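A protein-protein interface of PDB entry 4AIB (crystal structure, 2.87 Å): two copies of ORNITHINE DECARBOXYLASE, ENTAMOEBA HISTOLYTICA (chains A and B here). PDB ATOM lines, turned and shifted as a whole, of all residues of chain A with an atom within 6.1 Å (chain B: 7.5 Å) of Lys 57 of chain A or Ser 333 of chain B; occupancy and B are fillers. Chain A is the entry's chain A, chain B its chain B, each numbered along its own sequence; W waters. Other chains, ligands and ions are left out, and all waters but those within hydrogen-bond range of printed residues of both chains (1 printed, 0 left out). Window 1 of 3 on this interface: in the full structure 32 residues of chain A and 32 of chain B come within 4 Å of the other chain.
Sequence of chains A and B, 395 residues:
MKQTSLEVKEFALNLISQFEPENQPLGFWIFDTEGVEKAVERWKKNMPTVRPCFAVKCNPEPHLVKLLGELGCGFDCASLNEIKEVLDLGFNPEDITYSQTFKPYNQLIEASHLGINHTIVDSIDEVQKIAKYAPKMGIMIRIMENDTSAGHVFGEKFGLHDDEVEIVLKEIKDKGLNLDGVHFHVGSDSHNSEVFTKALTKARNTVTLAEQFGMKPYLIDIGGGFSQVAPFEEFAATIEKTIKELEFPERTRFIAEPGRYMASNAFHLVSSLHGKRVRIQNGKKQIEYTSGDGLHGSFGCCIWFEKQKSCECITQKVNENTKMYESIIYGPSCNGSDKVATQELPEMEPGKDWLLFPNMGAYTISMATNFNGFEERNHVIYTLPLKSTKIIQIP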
ATOM      1  N   PHE A  54     -12.723 -18.045  16.430  1.00  0.00           N
ATOM      2  CA  PHE A  54     -12.545 -17.307  15.182  1.00  0.00           C
ATOM      3  C   PHE A  54     -11.104 -16.866  14.951  1.00  0.00           C
ATOM      4  O   PHE A  54     -10.480 -16.258  15.825  1.00  0.00           O
ATOM      5  CB  PHE A  54     -13.485 -16.097  15.129  1.00  0.00           C
ATOM      6  CG  PHE A  54     -13.291 -15.227  13.915  1.00  0.00           C
ATOM      7  CD1 PHE A  54     -13.703 -15.659  12.657  1.00  0.00           C
ATOM      8  CD2 PHE A  54     -12.704 -13.970  14.031  1.00  0.00           C
ATOM      9  CE1 PHE A  54     -13.529 -14.858  11.539  1.00  0.00           C
ATOM     10  CE2 PHE A  54     -12.526 -13.165  12.916  1.00  0.00           C
ATOM     11  CZ  PHE A  54     -12.940 -13.609  11.668  1.00  0.00           C
ATOM     12  N   ALA A  55     -10.593 -17.181  13.764  1.00  0.00           N
ATOM     13  CA  ALA A  55      -9.279 -16.720  13.332  1.00  0.00           C
ATOM     14  C   ALA A  55      -9.345 -15.233  13.002  1.00  0.00           C
ATOM     15  O   ALA A  55      -9.837 -14.841  11.941  1.00  0.00           O
ATOM     16  CB  ALA A  55      -8.796 -17.524  12.133  1.00  0.00           C
ATOM     17  N   VAL A  56      -8.856 -14.414  13.933  1.00  0.00           N
ATOM     18  CA  VAL A  56      -8.863 -12.953  13.805  1.00  0.00           C
ATOM     19  C   VAL A  56      -8.079 -12.506  12.566  1.00  0.00           C
ATOM     20  O   VAL A  56      -8.373 -11.463  11.978  1.00  0.00           O
ATOM     21  CB  VAL A  56      -8.296 -12.270  15.076  1.00  0.00           C
ATOM     22  CG1 VAL A  56      -8.499 -10.761  15.026  1.00  0.00           C
ATOM     23  CG2 VAL A  56      -8.949 -12.838  16.329  1.00  0.00           C
ATOM     24  N   LYS A  57      -7.098 -13.318  12.173  1.00  0.00           N
ATOM     25  CA  LYS A  57      -6.265 -13.060  10.998  1.00  0.00           C
ATOM     26  C   LYS A  57      -7.075 -12.979   9.701  1.00  0.00           C
ATOM     27  O   LYS A  57      -6.736 -12.206   8.802  1.00  0.00           O
ATOM     28  CB  LYS A  57      -5.179 -14.135  10.876  1.00  0.00           C
ATOM     29  CG  LYS A  57      -4.018 -13.756   9.969  1.00  0.00           C
ATOM     30  CD  LYS A  57      -3.010 -14.889   9.857  1.00  0.00           C
ATOM     31  CE  LYS A  57      -1.803 -14.484   9.024  1.00  0.00           C
ATOM     32  NZ  LYS A  57      -2.125 -14.321   7.578  1.00  0.00           N
ATOM     33  N   CYS A  58      -8.140 -13.775   9.613  1.00  0.00           N
ATOM     34  CA  CYS A  58      -8.997 -13.804   8.429  1.00  0.00           C
ATOM     35  C   CYS A  58      -9.691 -12.461   8.193  1.00  0.00           C
ATOM     36  O   CYS A  58      -9.678 -11.939   7.076  1.00  0.00           O
ATOM     37  CB  CYS A  58     -10.026 -14.933   8.533  1.00  0.00           C
ATOM     38  SG  CYS A  58     -10.893 -15.281   6.986  1.00  0.00           S
ATOM     39  N   ASN A  59     -10.293 -11.912   9.248  1.00  0.00           N
ATOM     40  CA  ASN A  59     -10.913 -10.587   9.205  1.00  0.00           C
ATOM     41  C   ASN A  59     -10.937  -9.944  10.595  1.00  0.00           C
ATOM     42  O   ASN A  59     -11.786 -10.284  11.422  1.00  0.00           O
ATOM     43  CB  ASN A  59     -12.326 -10.661   8.613  1.00  0.00           C
ATOM     44  CG  ASN A  59     -12.838  -9.310   8.136  1.00  0.00           C
ATOM     45  OD1 ASN A  59     -12.446  -8.260   8.648  1.00  0.00           O
ATOM     46  ND2 ASN A  59     -13.726  -9.336   7.151  1.00  0.00           N
ATOM     47  N   PRO A  60      -9.997  -9.012  10.855  1.00  0.00           N
ATOM     48  CA  PRO A  60      -9.868  -8.376  12.167  1.00  0.00           C
ATOM     49  C   PRO A  60     -10.706  -7.101  12.356  1.00  0.00           C
ATOM     50  O   PRO A  60     -10.370  -6.271  13.207  1.00  0.00           O
ATOM     51  CB  PRO A  60      -8.373  -8.052  12.239  1.00  0.00           C
ATOM     52  CG  PRO A  60      -7.978  -7.814  10.821  1.00  0.00           C
ATOM     53  CD  PRO A  60      -8.912  -8.606   9.943  1.00  0.00           C
ATOM     54  N   ASP A  76      -8.799 -16.910  17.957  1.00  0.00           N
ATOM     55  CA  ASP A  76      -7.566 -17.468  17.426  1.00  0.00           C
ATOM     56  C   ASP A  76      -6.665 -16.340  16.927  1.00  0.00           C
ATOM     57  O   ASP A  76      -6.925 -15.735  15.884  1.00  0.00           O
ATOM     58  CB  ASP A  76      -7.885 -18.442  16.292  1.00  0.00           C
ATOM     59  CG  ASP A  76      -6.703 -19.298  15.914  1.00  0.00           C
ATOM     60  OD1 ASP A  76      -6.217 -20.047  16.785  1.00  0.00           O
ATOM     61  OD2 ASP A  76      -6.254 -19.217  14.752  1.00  0.00           O
ATOM     62  N   CYS A  77      -5.608 -16.057  17.681  1.00  0.00           N
ATOM     63  CA  CYS A  77      -4.741 -14.921  17.383  1.00  0.00           C
ATOM     64  C   CYS A  77      -3.347 -15.355  16.948  1.00  0.00           C
ATOM     65  O   CYS A  77      -2.694 -16.157  17.621  1.00  0.00           O
ATOM     66  CB  CYS A  77      -4.671 -13.979  18.585  1.00  0.00           C
ATOM     67  SG  CYS A  77      -6.285 -13.365  19.120  1.00  0.00           S
ATOM     68  N   ALA A  78      -2.906 -14.813  15.815  1.00  0.00           N
ATOM     69  CA  ALA A  78      -1.613 -15.157  15.225  1.00  0.00           C
ATOM     70  C   ALA A  78      -0.493 -14.239  15.707  1.00  0.00           C
ATOM     71  O   ALA A  78       0.645 -14.679  15.877  1.00  0.00           O
ATOM     72  CB  ALA A  78      -1.703 -15.135  13.706  1.00  0.00           C
ATOM     73  N   GLU A  82      -3.272  -8.905  17.166  1.00  0.00           N
ATOM     74  CA  GLU A  82      -4.542  -9.630  17.189  1.00  0.00           C
ATOM     75  C   GLU A  82      -4.954  -9.984  18.618  1.00  0.00           C
ATOM     76  O   GLU A  82      -6.140  -9.967  18.948  1.00  0.00           O
ATOM     77  CB  GLU A  82      -4.460 -10.897  16.335  1.00  0.00           C
ATOM     78  CG  GLU A  82      -4.380 -10.640  14.837  1.00  0.00           C
ATOM     79  CD  GLU A  82      -4.261 -11.914  14.016  1.00  0.00           C
ATOM     80  OE1 GLU A  82      -4.753 -12.975  14.462  1.00  0.00           O
ATOM     81  OE2 GLU A  82      -3.676 -11.850  12.915  1.00  0.00           O
ATOM     82  N   GLN A 100       0.469 -19.366  17.070  1.00  0.00           N
ATOM     83  CA  GLN A 100       1.645 -19.022  16.287  1.00  0.00           C
ATOM     84  C   GLN A 100       2.747 -20.028  16.584  1.00  0.00           C
ATOM     85  O   GLN A 100       3.225 -20.126  17.717  1.00  0.00           O
ATOM     86  CB  GLN A 100       2.100 -17.589  16.586  1.00  0.00           C
ATOM     87  CG  GLN A 100       3.313 -17.120  15.789  1.00  0.00           C
ATOM     88  CD  GLN A 100       3.136 -17.257  14.287  1.00  0.00           C
ATOM     89  OE1 GLN A 100       3.923 -17.928  13.619  1.00  0.00           O
ATOM     90  NE2 GLN A 100       2.099 -16.624  13.748  1.00  0.00           N
ATOM     91  N   PHE A 158       4.642 -26.350   7.948  1.00  0.00           N
ATOM     92  CA  PHE A 158       3.569 -26.192   8.943  1.00  0.00           C
ATOM     93  C   PHE A 158       3.040 -27.511   9.505  1.00  0.00           C
ATOM     94  O   PHE A 158       2.258 -28.217   8.861  1.00  0.00           O
ATOM     95  CB  PHE A 158       2.432 -25.293   8.430  1.00  0.00           C
ATOM     96  CG  PHE A 158       2.734 -23.825   8.534  1.00  0.00           C
ATOM     97  CD1 PHE A 158       2.572 -23.151   9.742  1.00  0.00           C
ATOM     98  CD2 PHE A 158       3.188 -23.114   7.428  1.00  0.00           C
ATOM     99  CE1 PHE A 158       2.853 -21.797   9.843  1.00  0.00           C
ATOM    100  CE2 PHE A 158       3.471 -21.758   7.523  1.00  0.00           C
ATOM    101  CZ  PHE A 158       3.305 -21.101   8.732  1.00  0.00           C
ATOM    102  N   TYR A 363     -10.848 -13.049   4.122  1.00  0.00           N
ATOM    103  CA  TYR A 363      -9.462 -12.718   3.743  1.00  0.00           C
ATOM    104  C   TYR A 363      -9.313 -11.466   2.864  1.00  0.00           C
ATOM    105  O   TYR A 363      -8.194 -10.996   2.638  1.00  0.00           O
ATOM    106  CB  TYR A 363      -8.741 -13.916   3.100  1.00  0.00           C
ATOM    107  CG  TYR A 363      -8.184 -14.918   4.089  1.00  0.00           C
ATOM    108  CD1 TYR A 363      -7.054 -14.620   4.853  1.00  0.00           C
ATOM    109  CD2 TYR A 363      -8.775 -16.172   4.249  1.00  0.00           C
ATOM    110  CE1 TYR A 363      -6.538 -15.536   5.757  1.00  0.00           C
ATOM    111  CE2 TYR A 363      -8.265 -17.095   5.151  1.00  0.00           C
ATOM    112  CZ  TYR A 363      -7.148 -16.773   5.901  1.00  0.00           C
ATOM    113  OH  TYR A 363      -6.640 -17.687   6.794  1.00  0.00           O
ATOM    114  N   TYR B 330      11.632 -18.359   6.329  1.00  0.00           N
ATOM    115  CA  TYR B 330      10.234 -17.960   6.175  1.00  0.00           C
ATOM    116  C   TYR B 330      10.000 -16.529   6.667  1.00  0.00           C
ATOM    117  O   TYR B 330      10.900 -15.901   7.234  1.00  0.00           O
ATOM    118  CB  TYR B 330       9.312 -18.940   6.911  1.00  0.00           C
ATOM    119  CG  TYR B 330       9.393 -20.372   6.417  1.00  0.00           C
ATOM    120  CD1 TYR B 330       8.818 -20.746   5.202  1.00  0.00           C
ATOM    121  CD2 TYR B 330      10.036 -21.354   7.170  1.00  0.00           C
ATOM    122  CE1 TYR B 330       8.889 -22.053   4.747  1.00  0.00           C
ATOM    123  CE2 TYR B 330      10.110 -22.666   6.724  1.00  0.00           C
ATOM    124  CZ  TYR B 330       9.534 -23.009   5.512  1.00  0.00           C
ATOM    125  OH  TYR B 330       9.603 -24.308   5.060  1.00  0.00           O
ATOM    126  N   GLY B 331       8.789 -16.023   6.440  1.00  0.00           N
ATOM    127  CA  GLY B 331       8.408 -14.678   6.867  1.00  0.00           C
ATOM    128  C   GLY B 331       7.123 -14.665   7.676  1.00  0.00           C
ATOM    129  O   GLY B 331       7.003 -15.404   8.656  1.00  0.00           O
ATOM    130  N   PRO B 332       6.154 -13.817   7.277  1.00  0.00           N
ATOM    131  CA  PRO B 332       4.849 -13.730   7.933  1.00  0.00           C
ATOM    132  C   PRO B 332       3.842 -14.745   7.379  1.00  0.00           C
ATOM    133  O   PRO B 332       4.210 -15.595   6.562  1.00  0.00           O
ATOM    134  CB  PRO B 332       4.387 -12.293   7.622  1.00  0.00           C
ATOM    135  CG  PRO B 332       5.459 -11.671   6.776  1.00  0.00           C
ATOM    136  CD  PRO B 332       6.292 -12.789   6.232  1.00  0.00           C
ATOM    137  N   SER B 333       2.591 -14.644   7.836  1.00  0.00           N
ATOM    138  CA  SER B 333       1.474 -15.505   7.408  1.00  0.00           C
ATOM    139  C   SER B 333       1.603 -16.962   7.866  1.00  0.00           C
ATOM    140  O   SER B 333       2.514 -17.682   7.448  1.00  0.00           O
ATOM    141  CB  SER B 333       1.241 -15.419   5.890  1.00  0.00           C
ATOM    142  OG  SER B 333       0.115 -16.185   5.497  1.00  0.00           O
ATOM    143  N   CYS B 334       0.680 -17.384   8.729  1.00  0.00           N
ATOM    144  CA  CYS B 334       0.645 -18.760   9.225  1.00  0.00           C
ATOM    145  C   CYS B 334      -0.310 -19.635   8.402  1.00  0.00           C
ATOM    146  O   CYS B 334      -1.234 -20.252   8.944  1.00  0.00           O
ATOM    147  CB  CYS B 334       0.304 -18.801  10.722  1.00  0.00           C
ATOM    148  SG  CYS B 334      -1.194 -17.910  11.203  1.00  0.00           S
ATOM    149  N   ASN B 335      -0.060 -19.680   7.092  1.00  0.00           N
ATOM    150  CA  ASN B 335      -0.852 -20.459   6.131  1.00  0.00           C
ATOM    151  C   ASN B 335      -2.348 -20.143   6.181  1.00  0.00           C
ATOM    152  O   ASN B 335      -2.793 -19.123   5.656  1.00  0.00           O
ATOM    153  CB  ASN B 335      -0.606 -21.965   6.307  1.00  0.00           C
ATOM    154  CG  ASN B 335      -1.003 -22.776   5.084  1.00  0.00           C
ATOM    155  OD1 ASN B 335      -2.182 -22.879   4.745  1.00  0.00           O
ATOM    156  ND2 ASN B 335      -0.015 -23.369   4.426  1.00  0.00           N
ATOM    157  N   ASP B 338       5.516 -15.907   2.068  1.00  0.00           N
ATOM    158  CA  ASP B 338       5.619 -16.919   3.114  1.00  0.00           C
ATOM    159  C   ASP B 338       6.966 -17.645   3.071  1.00  0.00           C
ATOM    160  O   ASP B 338       7.431 -18.163   4.087  1.00  0.00           O
ATOM    161  CB  ASP B 338       4.463 -17.922   3.005  1.00  0.00           C
ATOM    162  CG  ASP B 338       4.272 -18.751   4.272  1.00  0.00           C
ATOM    163  OD1 ASP B 338       4.577 -18.258   5.381  1.00  0.00           O
ATOM    164  OD2 ASP B 338       3.802 -19.901   4.157  1.00  0.00           O
HETATM  165  O   HOH W   1       3.288 -17.174  10.773  1.00  0.00           O
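The side-chain carboxylate of Glu 82 of chain A is in hydrogen-bond range of the backbone NH of Lys 57 of chain A, at 3.3 Å. The backbone NH of Ala 78 of chain A is in hydrogen-bond range of the side-chain carboxylate of Glu 82 of chain A (2.9 Å). NE2 of Gln 100 of chain A lies within hydrogen-bond range of O of Ala 78 of chain A (3.2 Å). N of Gly 331 of chain B sits at hydrogen-bond distance from O of Asp 338 of chain B, 3.5 Å away.
Among the printed residues, pairs that only touch across the chains: Lys 57 of chain A with Ser 333 of chain B (3.6 Å), Lys 57 of chain A with Cys 334 of chain B (3.8 Å), Ala 78 of chain A with Cys 334 of chain B (3.8 Å), Phe 158 of chain A with Ser 333 of chain B (3.7 Å), Phe 158 of chain A with Cys 334 of chain B (3.6 Å) and Phe 158 of chain A with Asp 338 of chain B (3.9 Å).
Lys 57 of chain A touches two residues of chain B. Printed residues of chain B within 4 Å of Ala 78 of chain A: Cys 334. Glu 82 of chain A touches none of the printed residues of chain B. Of the printed residues of chain B, Phe 158 of chain A touches Ser 333, Cys 334 and Asp 338. Tyr 330 of chain B touches none of the printed residues of chain A. Ser 333 of chain B touches just these residues of chain A: Lys 57 and Phe 158. Of the printed residues of chain A, Cys 334 of chain B touches Lys 57, Ala 78 and Phe 158. Of the printed residues of chain A, Asp 338 of chain B touches Phe 158. The nearest residue of chain A that does not touch Ser 333 of chain B is Gln 100 of chain A (5.9 Å).
Hydrophobic or aromatic side chains of chain A that line the printed part of chain B: Ala 78 and Phe 158. Printed residues of chain B that touch a printed residue of chain A: Ser 333, Cys 334 and Asp 338. Among the printed residues, 6 pairs touch across the chains.
No position is printed for both chains. Of the 6 pairs that touch across the chains among the printed residues, none has its exchanged pair printed and touching as well.
Water W1 lies within hydrogen-bond range of OE1 of Gln 100 of chain A (3.0 Å), N of Cys 334 of chain B (3.3 Å) and O of Ser 333 of chain B (3.5 Å).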
